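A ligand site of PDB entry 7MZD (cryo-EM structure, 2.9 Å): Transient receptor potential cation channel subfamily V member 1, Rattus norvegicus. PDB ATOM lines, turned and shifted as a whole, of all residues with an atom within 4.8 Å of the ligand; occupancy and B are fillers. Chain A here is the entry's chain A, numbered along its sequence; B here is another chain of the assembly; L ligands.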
ATOM      1  N   PHE A 403       9.568  -4.401  28.843  1.00  0.00           N
ATOM      2  CA  PHE A 403       8.896  -4.563  27.551  1.00  0.00           C
ATOM      3  C   PHE A 403       8.858  -6.008  27.063  1.00  0.00           C
ATOM      4  O   PHE A 403       7.842  -6.441  26.529  1.00  0.00           O
ATOM      5  CB  PHE A 403       9.571  -3.698  26.497  1.00  0.00           C
ATOM      6  CG  PHE A 403       9.205  -2.252  26.588  1.00  0.00           C
ATOM      7  CD1 PHE A 403       8.108  -1.759  25.919  1.00  0.00           C
ATOM      8  CD2 PHE A 403       9.967  -1.383  27.345  1.00  0.00           C
ATOM      9  CE1 PHE A 403       7.761  -0.430  26.000  1.00  0.00           C
ATOM     10  CE2 PHE A 403       9.625  -0.047  27.438  1.00  0.00           C
ATOM     11  CZ  PHE A 403       8.528   0.431  26.761  1.00  0.00           C
ATOM     12  N   TYR A 407       4.079  -6.818  28.554  1.00  0.00           N
ATOM     13  CA  TYR A 407       3.759  -6.026  27.365  1.00  0.00           C
ATOM     14  C   TYR A 407       2.314  -5.545  27.382  1.00  0.00           C
ATOM     15  O   TYR A 407       2.034  -4.352  27.176  1.00  0.00           O
ATOM     16  CB  TYR A 407       4.054  -6.880  26.133  1.00  0.00           C
ATOM     17  CG  TYR A 407       3.759  -6.242  24.799  1.00  0.00           C
ATOM     18  CD1 TYR A 407       4.579  -5.273  24.270  1.00  0.00           C
ATOM     19  CD2 TYR A 407       2.667  -6.655  24.057  1.00  0.00           C
ATOM     20  CE1 TYR A 407       4.311  -4.705  23.043  1.00  0.00           C
ATOM     21  CE2 TYR A 407       2.396  -6.100  22.831  1.00  0.00           C
ATOM     22  CZ  TYR A 407       3.216  -5.127  22.336  1.00  0.00           C
ATOM     23  OH  TYR A 407       2.941  -4.565  21.106  1.00  0.00           O
ATOM     24  N   SER A 408       1.379  -6.462  27.633  1.00  0.00           N
ATOM     25  CA  SER A 408      -0.031  -6.095  27.625  1.00  0.00           C
ATOM     26  C   SER A 408      -0.368  -5.104  28.729  1.00  0.00           C
ATOM     27  O   SER A 408      -1.201  -4.219  28.531  1.00  0.00           O
ATOM     28  CB  SER A 408      -0.898  -7.351  27.759  1.00  0.00           C
ATOM     29  OG  SER A 408      -0.536  -8.077  28.908  1.00  0.00           O
ATOM     30  N   ILE A 410       1.598  -2.784  29.821  1.00  0.00           N
ATOM     31  CA  ILE A 410       2.036  -1.489  29.325  1.00  0.00           C
ATOM     32  C   ILE A 410       1.036  -0.937  28.329  1.00  0.00           C
ATOM     33  O   ILE A 410       0.738   0.261  28.338  1.00  0.00           O
ATOM     34  CB  ILE A 410       3.439  -1.597  28.688  1.00  0.00           C
ATOM     35  CG1 ILE A 410       4.475  -1.735  29.787  1.00  0.00           C
ATOM     36  CG2 ILE A 410       3.748  -0.347  27.852  1.00  0.00           C
ATOM     37  CD1 ILE A 410       5.775  -2.262  29.322  1.00  0.00           C
ATOM     38  N   LEU A 411       0.532  -1.773  27.423  1.00  0.00           N
ATOM     39  CA  LEU A 411      -0.417  -1.263  26.437  1.00  0.00           C
ATOM     40  C   LEU A 411      -1.691  -0.753  27.098  1.00  0.00           C
ATOM     41  O   LEU A 411      -2.188   0.328  26.751  1.00  0.00           O
ATOM     42  CB  LEU A 411      -0.730  -2.340  25.404  1.00  0.00           C
ATOM     43  CG  LEU A 411       0.403  -2.760  24.467  1.00  0.00           C
ATOM     44  CD1 LEU A 411      -0.088  -3.844  23.545  1.00  0.00           C
ATOM     45  CD2 LEU A 411       0.948  -1.577  23.663  1.00  0.00           C
ATOM     46  N   PHE A 412      -2.212  -1.483  28.080  1.00  0.00           N
ATOM     47  CA  PHE A 412      -3.402  -1.020  28.779  1.00  0.00           C
ATOM     48  C   PHE A 412      -3.115   0.264  29.551  1.00  0.00           C
ATOM     49  O   PHE A 412      -3.939   1.190  29.561  1.00  0.00           O
ATOM     50  CB  PHE A 412      -3.924  -2.108  29.706  1.00  0.00           C
ATOM     51  CG  PHE A 412      -4.820  -3.100  29.049  1.00  0.00           C
ATOM     52  CD1 PHE A 412      -6.152  -2.807  28.824  1.00  0.00           C
ATOM     53  CD2 PHE A 412      -4.341  -4.330  28.636  1.00  0.00           C
ATOM     54  CE1 PHE A 412      -6.985  -3.709  28.209  1.00  0.00           C
ATOM     55  CE2 PHE A 412      -5.175  -5.231  28.022  1.00  0.00           C
ATOM     56  CZ  PHE A 412      -6.494  -4.925  27.810  1.00  0.00           C
ATOM     57  N   PHE A 439      -6.313   8.167  19.765  1.00  0.00           N
ATOM     58  CA  PHE A 439      -5.236   7.206  19.991  1.00  0.00           C
ATOM     59  C   PHE A 439      -5.669   6.153  20.996  1.00  0.00           C
ATOM     60  O   PHE A 439      -5.579   4.960  20.712  1.00  0.00           O
ATOM     61  CB  PHE A 439      -3.968   7.897  20.470  1.00  0.00           C
ATOM     62  CG  PHE A 439      -3.132   8.478  19.363  1.00  0.00           C
ATOM     63  CD1 PHE A 439      -2.563   7.668  18.403  1.00  0.00           C
ATOM     64  CD2 PHE A 439      -2.885   9.834  19.316  1.00  0.00           C
ATOM     65  CE1 PHE A 439      -1.802   8.206  17.394  1.00  0.00           C
ATOM     66  CE2 PHE A 439      -2.111  10.370  18.314  1.00  0.00           C
ATOM     67  CZ  PHE A 439      -1.566   9.558  17.354  1.00  0.00           C
ATOM     68  N   ALA A 442      -8.023   3.774  19.335  1.00  0.00           N
ATOM     69  CA  ALA A 442      -7.340   2.794  18.511  1.00  0.00           C
ATOM     70  C   ALA A 442      -6.700   1.729  19.380  1.00  0.00           C
ATOM     71  O   ALA A 442      -6.935   0.529  19.196  1.00  0.00           O
ATOM     72  CB  ALA A 442      -6.281   3.473  17.641  1.00  0.00           C
ATOM     73  N   MET A 443      -5.977   2.161  20.432  1.00  0.00           N
ATOM     74  CA  MET A 443      -5.344   1.195  21.309  1.00  0.00           C
ATOM     75  C   MET A 443      -6.392   0.345  21.988  1.00  0.00           C
ATOM     76  O   MET A 443      -6.227  -0.878  22.103  1.00  0.00           O
ATOM     77  CB  MET A 443      -4.472   1.915  22.330  1.00  0.00           C
ATOM     78  CG  MET A 443      -3.310   2.660  21.716  1.00  0.00           C
ATOM     79  SD  MET A 443      -2.144   3.286  22.927  1.00  0.00           S
ATOM     80  CE  MET A 443      -1.397   1.763  23.489  1.00  0.00           C
ATOM     81  N   THR A 446      -7.093  -2.500  19.717  1.00  0.00           N
ATOM     82  CA  THR A 446      -6.009  -3.452  19.484  1.00  0.00           C
ATOM     83  C   THR A 446      -5.709  -4.261  20.735  1.00  0.00           C
ATOM     84  O   THR A 446      -5.311  -5.421  20.640  1.00  0.00           O
ATOM     85  CB  THR A 446      -4.764  -2.732  18.981  1.00  0.00           C
ATOM     86  OG1 THR A 446      -4.402  -1.695  19.900  1.00  0.00           O
ATOM     87  CG2 THR A 446      -5.034  -2.118  17.620  1.00  0.00           C
ATOM     88  N   ASN A 447      -5.970  -3.687  21.912  1.00  0.00           N
ATOM     89  CA  ASN A 447      -5.816  -4.422  23.147  1.00  0.00           C
ATOM     90  C   ASN A 447      -6.813  -5.572  23.265  1.00  0.00           C
ATOM     91  O   ASN A 447      -6.650  -6.395  24.176  1.00  0.00           O
ATOM     92  CB  ASN A 447      -5.971  -3.478  24.333  1.00  0.00           C
ATOM     93  CG  ASN A 447      -4.822  -2.506  24.448  1.00  0.00           C
ATOM     94  OD1 ASN A 447      -3.728  -2.754  23.948  1.00  0.00           O
ATOM     95  ND2 ASN A 447      -5.062  -1.395  25.120  1.00  0.00           N
ATOM     96  N   LEU A 449      -6.615  -7.961  21.448  1.00  0.00           N
ATOM     97  CA  LEU A 449      -5.741  -9.112  21.243  1.00  0.00           C
ATOM     98  C   LEU A 449      -5.259  -9.705  22.562  1.00  0.00           C
ATOM     99  O   LEU A 449      -4.909 -10.884  22.584  1.00  0.00           O
ATOM    100  CB  LEU A 449      -4.541  -8.718  20.389  1.00  0.00           C
ATOM    101  CG  LEU A 449      -4.722  -8.959  18.891  1.00  0.00           C
ATOM    102  CD1 LEU A 449      -5.831  -8.081  18.343  1.00  0.00           C
ATOM    103  CD2 LEU A 449      -3.426  -8.725  18.162  1.00  0.00           C
ATOM    104  N   TYR A 450      -5.246  -8.926  23.649  1.00  0.00           N
ATOM    105  CA  TYR A 450      -4.901  -9.477  24.952  1.00  0.00           C
ATOM    106  C   TYR A 450      -5.768 -10.675  25.287  1.00  0.00           C
ATOM    107  O   TYR A 450      -5.293 -11.652  25.881  1.00  0.00           O
ATOM    108  CB  TYR A 450      -5.036  -8.430  26.046  1.00  0.00           C
ATOM    109  CG  TYR A 450      -5.028  -9.016  27.428  1.00  0.00           C
ATOM    110  CD1 TYR A 450      -3.852  -9.444  28.016  1.00  0.00           C
ATOM    111  CD2 TYR A 450      -6.209  -9.163  28.156  1.00  0.00           C
ATOM    112  CE1 TYR A 450      -3.838  -9.985  29.278  1.00  0.00           C
ATOM    113  CE2 TYR A 450      -6.195  -9.705  29.418  1.00  0.00           C
ATOM    114  CZ  TYR A 450      -5.016 -10.122  29.972  1.00  0.00           C
ATOM    115  OH  TYR A 450      -5.002 -10.663  31.234  1.00  0.00           O
ATOM    116  N   ARG A 453      -5.513 -14.974  24.421  1.00  0.00           N
ATOM    117  CA  ARG A 453      -5.129 -16.056  25.311  1.00  0.00           C
ATOM    118  C   ARG A 453      -6.385 -16.700  25.882  1.00  0.00           C
ATOM    119  O   ARG A 453      -7.394 -16.031  26.135  1.00  0.00           O
ATOM    120  CB  ARG A 453      -4.238 -15.537  26.432  1.00  0.00           C
ATOM    121  CG  ARG A 453      -4.911 -14.574  27.389  1.00  0.00           C
ATOM    122  CD  ARG A 453      -3.886 -13.838  28.241  1.00  0.00           C
ATOM    123  NE  ARG A 453      -3.045 -12.962  27.439  1.00  0.00           N
ATOM    124  CZ  ARG A 453      -1.954 -12.344  27.888  1.00  0.00           C
ATOM    125  NH1 ARG A 453      -1.525 -12.498  29.129  1.00  0.00           N
ATOM    126  NH2 ARG A 453      -1.265 -11.562  27.061  1.00  0.00           N
ATOM    127  N   ALA A 462      -1.377 -13.969  18.294  1.00  0.00           N
ATOM    128  CA  ALA A 462      -1.139 -12.709  18.994  1.00  0.00           C
ATOM    129  C   ALA A 462       0.266 -12.668  19.582  1.00  0.00           C
ATOM    130  O   ALA A 462       0.913 -11.611  19.593  1.00  0.00           O
ATOM    131  CB  ALA A 462      -2.176 -12.523  20.106  1.00  0.00           C
ATOM    132  N   ILE A 465       2.613 -11.764  16.880  1.00  0.00           N
ATOM    133  CA  ILE A 465       2.566 -10.332  16.603  1.00  0.00           C
ATOM    134  C   ILE A 465       3.383  -9.558  17.643  1.00  0.00           C
ATOM    135  O   ILE A 465       4.175  -8.671  17.311  1.00  0.00           O
ATOM    136  CB  ILE A 465       1.115  -9.834  16.557  1.00  0.00           C
ATOM    137  CG1 ILE A 465       0.376 -10.432  15.356  1.00  0.00           C
ATOM    138  CG2 ILE A 465       1.071  -8.315  16.486  1.00  0.00           C
ATOM    139  CD1 ILE A 465      -1.118 -10.432  15.504  1.00  0.00           C
ATOM    140  N   GLU A 466       3.186  -9.903  18.910  1.00  0.00           N
ATOM    141  CA  GLU A 466       3.904  -9.224  19.994  1.00  0.00           C
ATOM    142  C   GLU A 466       5.406  -9.354  19.823  1.00  0.00           C
ATOM    143  O   GLU A 466       6.150  -8.371  19.930  1.00  0.00           O
ATOM    144  CB  GLU A 466       3.450  -9.794  21.341  1.00  0.00           C
ATOM    145  CG  GLU A 466       4.311  -9.433  22.550  1.00  0.00           C
ATOM    146  CD  GLU A 466       3.740  -9.939  23.851  1.00  0.00           C
ATOM    147  OE1 GLU A 466       2.588 -10.443  23.843  1.00  0.00           O
ATOM    148  OE2 GLU A 466       4.433  -9.855  24.878  1.00  0.00           O
ATOM    149  N   ILE A 469       6.823  -7.359  16.900  1.00  0.00           N
ATOM    150  CA  ILE A 469       6.986  -5.937  17.192  1.00  0.00           C
ATOM    151  C   ILE A 469       8.180  -5.717  18.114  1.00  0.00           C
ATOM    152  O   ILE A 469       9.010  -4.837  17.879  1.00  0.00           O
ATOM    153  CB  ILE A 469       5.690  -5.368  17.796  1.00  0.00           C
ATOM    154  CG1 ILE A 469       4.622  -5.264  16.713  1.00  0.00           C
ATOM    155  CG2 ILE A 469       5.939  -3.986  18.428  1.00  0.00           C
ATOM    156  CD1 ILE A 469       3.219  -5.050  17.235  1.00  0.00           C
ATOM    157  N   LEU A 473      11.030  -5.535  14.717  1.00  0.00           N
ATOM    158  CA  LEU A 473      10.547  -4.354  14.017  1.00  0.00           C
ATOM    159  C   LEU A 473      11.616  -3.266  13.923  1.00  0.00           C
ATOM    160  O   LEU A 473      11.752  -2.608  12.893  1.00  0.00           O
ATOM    161  CB  LEU A 473       9.297  -3.812  14.693  1.00  0.00           C
ATOM    162  CG  LEU A 473       8.609  -2.609  14.040  1.00  0.00           C
ATOM    163  CD1 LEU A 473       8.105  -2.958  12.654  1.00  0.00           C
ATOM    164  CD2 LEU A 473       7.473  -2.114  14.902  1.00  0.00           C
ATOM    165  N   GLN A 573       1.581 -17.212  29.276  1.00  0.00           N
ATOM    166  CA  GLN A 573       0.658 -16.092  29.421  1.00  0.00           C
ATOM    167  C   GLN A 573      -0.665 -16.544  30.030  1.00  0.00           C
ATOM    168  O   GLN A 573      -1.232 -15.856  30.884  1.00  0.00           O
ATOM    169  CB  GLN A 573       0.427 -15.429  28.066  1.00  0.00           C
ATOM    170  CG  GLN A 573       1.608 -14.618  27.570  1.00  0.00           C
ATOM    171  CD  GLN A 573       1.332 -13.940  26.247  1.00  0.00           C
ATOM    172  OE1 GLN A 573       0.351 -14.250  25.566  1.00  0.00           O
ATOM    173  NE2 GLN A 573       2.196 -13.010  25.870  1.00  0.00           N
ATOM    174  N   PHE B 483      -8.021  -4.915  14.081  1.00  0.00           N
ATOM    175  CA  PHE B 483      -7.146  -3.800  13.746  1.00  0.00           C
ATOM    176  C   PHE B 483      -7.850  -2.804  12.830  1.00  0.00           C
ATOM    177  O   PHE B 483      -7.791  -1.583  13.053  1.00  0.00           O
ATOM    178  CB  PHE B 483      -5.869  -4.318  13.089  1.00  0.00           C
ATOM    179  CG  PHE B 483      -4.805  -4.697  14.064  1.00  0.00           C
ATOM    180  CD1 PHE B 483      -4.927  -5.852  14.808  1.00  0.00           C
ATOM    181  CD2 PHE B 483      -3.694  -3.915  14.238  1.00  0.00           C
ATOM    182  CE1 PHE B 483      -3.954  -6.215  15.715  1.00  0.00           C
ATOM    183  CE2 PHE B 483      -2.718  -4.264  15.144  1.00  0.00           C
ATOM    184  CZ  PHE B 483      -2.848  -5.418  15.873  1.00  0.00           C
ATOM    185  N   PHE B 487      -8.709   1.158  13.934  1.00  0.00           N
ATOM    186  CA  PHE B 487      -8.145   2.322  13.278  1.00  0.00           C
ATOM    187  C   PHE B 487      -9.204   3.087  12.487  1.00  0.00           C
ATOM    188  O   PHE B 487      -9.116   4.317  12.384  1.00  0.00           O
ATOM    189  CB  PHE B 487      -6.972   1.910  12.392  1.00  0.00           C
ATOM    190  CG  PHE B 487      -5.708   1.713  13.159  1.00  0.00           C
ATOM    191  CD1 PHE B 487      -4.879   2.778  13.421  1.00  0.00           C
ATOM    192  CD2 PHE B 487      -5.359   0.464  13.634  1.00  0.00           C
ATOM    193  CE1 PHE B 487      -3.719   2.610  14.134  1.00  0.00           C
ATOM    194  CE2 PHE B 487      -4.199   0.297  14.348  1.00  0.00           C
ATOM    195  CZ  PHE B 487      -3.383   1.364  14.603  1.00  0.00           C
ATOM    196  N   LEU B 535      -1.858   7.862  12.329  1.00  0.00           N
ATOM    197  CA  LEU B 535      -2.788   6.735  12.417  1.00  0.00           C
ATOM    198  C   LEU B 535      -2.738   5.885  11.161  1.00  0.00           C
ATOM    199  O   LEU B 535      -2.696   4.655  11.245  1.00  0.00           O
ATOM    200  CB  LEU B 535      -4.212   7.234  12.653  1.00  0.00           C
ATOM    201  CG  LEU B 535      -4.571   7.741  14.058  1.00  0.00           C
ATOM    202  CD1 LEU B 535      -5.913   8.418  14.032  1.00  0.00           C
ATOM    203  CD2 LEU B 535      -4.568   6.601  15.057  1.00  0.00           C
ATOM    204  N   ALA B 538       0.610   3.949  10.995  1.00  0.00           N
ATOM    205  CA  ALA B 538       0.619   2.865  11.973  1.00  0.00           C
ATOM    206  C   ALA B 538      -0.270   1.722  11.511  1.00  0.00           C
ATOM    207  O   ALA B 538       0.098   0.551  11.662  1.00  0.00           O
ATOM    208  CB  ALA B 538       0.165   3.384  13.332  1.00  0.00           C
ATOM    209  N   ILE B 541       1.611  -0.216   8.722  1.00  0.00           N
ATOM    210  CA  ILE B 541       2.722  -1.034   9.212  1.00  0.00           C
ATOM    211  C   ILE B 541       2.202  -2.226   9.995  1.00  0.00           C
ATOM    212  O   ILE B 541       2.692  -3.350   9.844  1.00  0.00           O
ATOM    213  CB  ILE B 541       3.685  -0.172  10.063  1.00  0.00           C
ATOM    214  CG1 ILE B 541       4.369   0.879   9.184  1.00  0.00           C
ATOM    215  CG2 ILE B 541       4.722  -1.053  10.736  1.00  0.00           C
ATOM    216  CD1 ILE B 541       4.971   2.028   9.963  1.00  0.00           C
ATOM    217  N   LEU B 542       1.189  -2.009  10.830  1.00  0.00           N
ATOM    218  CA  LEU B 542       0.625  -3.117  11.608  1.00  0.00           C
ATOM    219  C   LEU B 542      -0.035  -4.139  10.696  1.00  0.00           C
ATOM    220  O   LEU B 542       0.049  -5.341  10.949  1.00  0.00           O
ATOM    221  CB  LEU B 542      -0.360  -2.571  12.640  1.00  0.00           C
ATOM    222  CG  LEU B 542       0.252  -1.755  13.768  1.00  0.00           C
ATOM    223  CD1 LEU B 542      -0.812  -0.983  14.511  1.00  0.00           C
ATOM    224  CD2 LEU B 542       1.023  -2.647  14.725  1.00  0.00           C
ATOM    225  N   ILE B 545       2.619  -6.213   9.211  1.00  0.00           N
ATOM    226  CA  ILE B 545       3.085  -7.148  10.241  1.00  0.00           C
ATOM    227  C   ILE B 545       2.112  -8.318  10.364  1.00  0.00           C
ATOM    228  O   ILE B 545       2.532  -9.477  10.480  1.00  0.00           O
ATOM    229  CB  ILE B 545       3.252  -6.414  11.577  1.00  0.00           C
ATOM    230  CG1 ILE B 545       4.471  -5.486  11.520  1.00  0.00           C
ATOM    231  CG2 ILE B 545       3.395  -7.405  12.730  1.00  0.00           C
ATOM    232  CD1 ILE B 545       4.503  -4.440  12.600  1.00  0.00           C
HETATM  233  C1  LIG L   1      -2.670  -5.702  25.097  1.00  0.00           C
HETATM  234  O1  LIG L   1      -2.005  -6.929  24.970  1.00  0.00           O
HETATM  235  C2  LIG L   1      -1.683  -7.270  23.646  1.00  0.00           C
HETATM  236  C3  LIG L   1      -2.018  -6.459  22.670  1.00  0.00           C
HETATM  237  C4  LIG L   1      -0.944  -8.564  23.344  1.00  0.00           C
HETATM  238  O2  LIG L   1      -0.586  -9.424  24.397  1.00  0.00           O
HETATM  239  C5  LIG L   1      -0.630  -8.879  22.110  1.00  0.00           C
HETATM  240  C6  LIG L   1      -1.016  -7.940  20.970  1.00  0.00           C
HETATM  241  C7  LIG L   1      -1.660  -6.822  21.232  1.00  0.00           C
HETATM  242  C8  LIG L   1      -2.054  -5.866  20.085  1.00  0.00           C
HETATM  243  C9  LIG L   1      -0.792  -5.145  19.567  1.00  0.00           C
HETATM  244  O3  LIG L   1       0.262  -5.367  20.053  1.00  0.00           O
HETATM  245  O4  LIG L   1      -0.891  -4.191  18.520  1.00  0.00           O
HETATM  246  C10 LIG L   1       0.356  -3.608  18.195  1.00  0.00           C
HETATM  247  C11 LIG L   1       0.323  -2.130  18.677  1.00  0.00           C
HETATM  248  C12 LIG L   1       1.471  -1.488  18.798  1.00  0.00           C
HETATM  249  C13 LIG L   1       1.773  -0.650  19.993  1.00  0.00           C
HETATM  250  C14 LIG L   1      -0.988  -1.347  18.474  1.00  0.00           C
HETATM  251  C15 LIG L   1      -0.950   0.131  19.056  1.00  0.00           C
HETATM  252  O5  LIG L   1      -1.002   0.105  20.441  1.00  0.00           O
HETATM  253  C16 LIG L   1      -2.099   0.877  18.564  1.00  0.00           C
HETATM  254  O6  LIG L   1      -3.206   0.477  18.464  1.00  0.00           O
HETATM  255  C17 LIG L   1      -1.584   2.334  18.190  1.00  0.00           C
HETATM  256  C18 LIG L   1      -2.445   3.558  17.936  1.00  0.00           C
HETATM  257  C19 LIG L   1      -0.149   2.279  18.151  1.00  0.00           C
HETATM  258  C20 LIG L   1       0.267   0.836  18.555  1.00  0.00           C
HETATM  259  C21 LIG L   1       1.370   0.895  19.606  1.00  0.00           C
HETATM  260  O7  LIG L   1       2.661   1.517  18.843  1.00  0.00           O
HETATM  261  C22 LIG L   1       1.472   1.720  20.869  1.00  0.00           C
HETATM  262  C23 LIG L   1       1.925   3.122  20.580  1.00  0.00           C
HETATM  263  C24 LIG L   1       2.453   1.032  21.910  1.00  0.00           C
HETATM  264  C25 LIG L   1       3.656   0.410  21.197  1.00  0.00           C
HETATM  265  C26 LIG L   1       4.656  -0.139  22.227  1.00  0.00           C
HETATM  266  C27 LIG L   1       5.325  -1.426  21.812  1.00  0.00           C
HETATM  267  C28 LIG L   1       4.103  -0.159  23.650  1.00  0.00           C
HETATM  268  O8  LIG L   1       4.214   1.227  20.516  1.00  0.00           O
HETATM  269  C29 LIG L   1       3.195  -0.716  20.230  1.00  0.00           C
HETATM  270  O9  LIG L   1       3.715  -0.446  19.139  1.00  0.00           O
HETATM  271  C30 LIG L   1       3.855   0.857  19.156  1.00  0.00           C
HETATM  272  C31 LIG L   1       4.947   1.256  18.150  1.00  0.00           C
HETATM  273  C32 LIG L   1       4.451   0.903  16.747  1.00  0.00           C
HETATM  274  C33 LIG L   1       3.870   1.820  16.016  1.00  0.00           C
HETATM  275  C34 LIG L   1       3.379   1.459  14.617  1.00  0.00           C
HETATM  276  C35 LIG L   1       3.538   0.243  14.156  1.00  0.00           C
HETATM  277  C36 LIG L   1       4.215  -0.811  15.006  1.00  0.00           C
HETATM  278  C37 LIG L   1       4.641  -0.505  16.208  1.00  0.00           C
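NH2 of Arg 453 lies within hydrogen-bond range of O2 of the ligand (3.5 Å).
O2 of the ligand lies within hydrogen-bond range of OE1 of Glu 466 (3.4 Å).
OG1 of Thr 446 is in hydrogen-bond range of O6 of the ligand, 2.9 Å away.
OH of Tyr 407 sits at hydrogen-bond distance from O3 of the ligand.
The side-chain hydroxyl (OG1) of Thr 446 lies within hydrogen-bond range of the backbone carbonyl oxygen (O) of Met 443 (3.0 Å).
The backbone carbonyl oxygen (O) of Met 443 sits close to the side-chain amide nitrogen (ND2) of Asn 447 (3.3 Å).
O of Ala 442 is in hydrogen-bond range of OG1 of Thr 446, at 3.4 Å.
OE1 of Glu 466 sits at hydrogen-bond distance from NE2 of Gln 573 (3.3 Å).
NH2 of Arg 453 lies within hydrogen-bond range of OE1 of Gln 573 (3.5 Å).
NE of Arg 453 sits at hydrogen-bond distance from O of Tyr 450, at 3.0 Å.
Residues that only touch the ligand: Ser 408 (3.0 Å), Asn 447 (3.3 Å), Ile 469 (3.3 Å), Leu 411 (3.4 Å), Met 443 (3.5 Å), Leu 473 (3.5 Å), Phe 483 of chain B (3.5 Å), Tyr 450 (3.5 Å), Leu 449 (3.6 Å), Leu 542 of chain B (3.7 Å), Ala 442 (3.8 Å), Ile 541 of chain B (3.8 Å), Phe 412 (3.9 Å), Ala 538 of chain B (3.96 Å) and Phe 487 of chain B (3.97 Å).
Hydrophobic or aromatic side chains that line the ligand: Tyr 407, Leu 411, Phe 412, Ala 442, Met 443, Leu 449, Tyr 450, Ile 469, Leu 473, Phe 483 of chain B, Phe 487 of chain B, Ala 538 of chain B, Ile 541 of chain B and Leu 542 of chain B.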
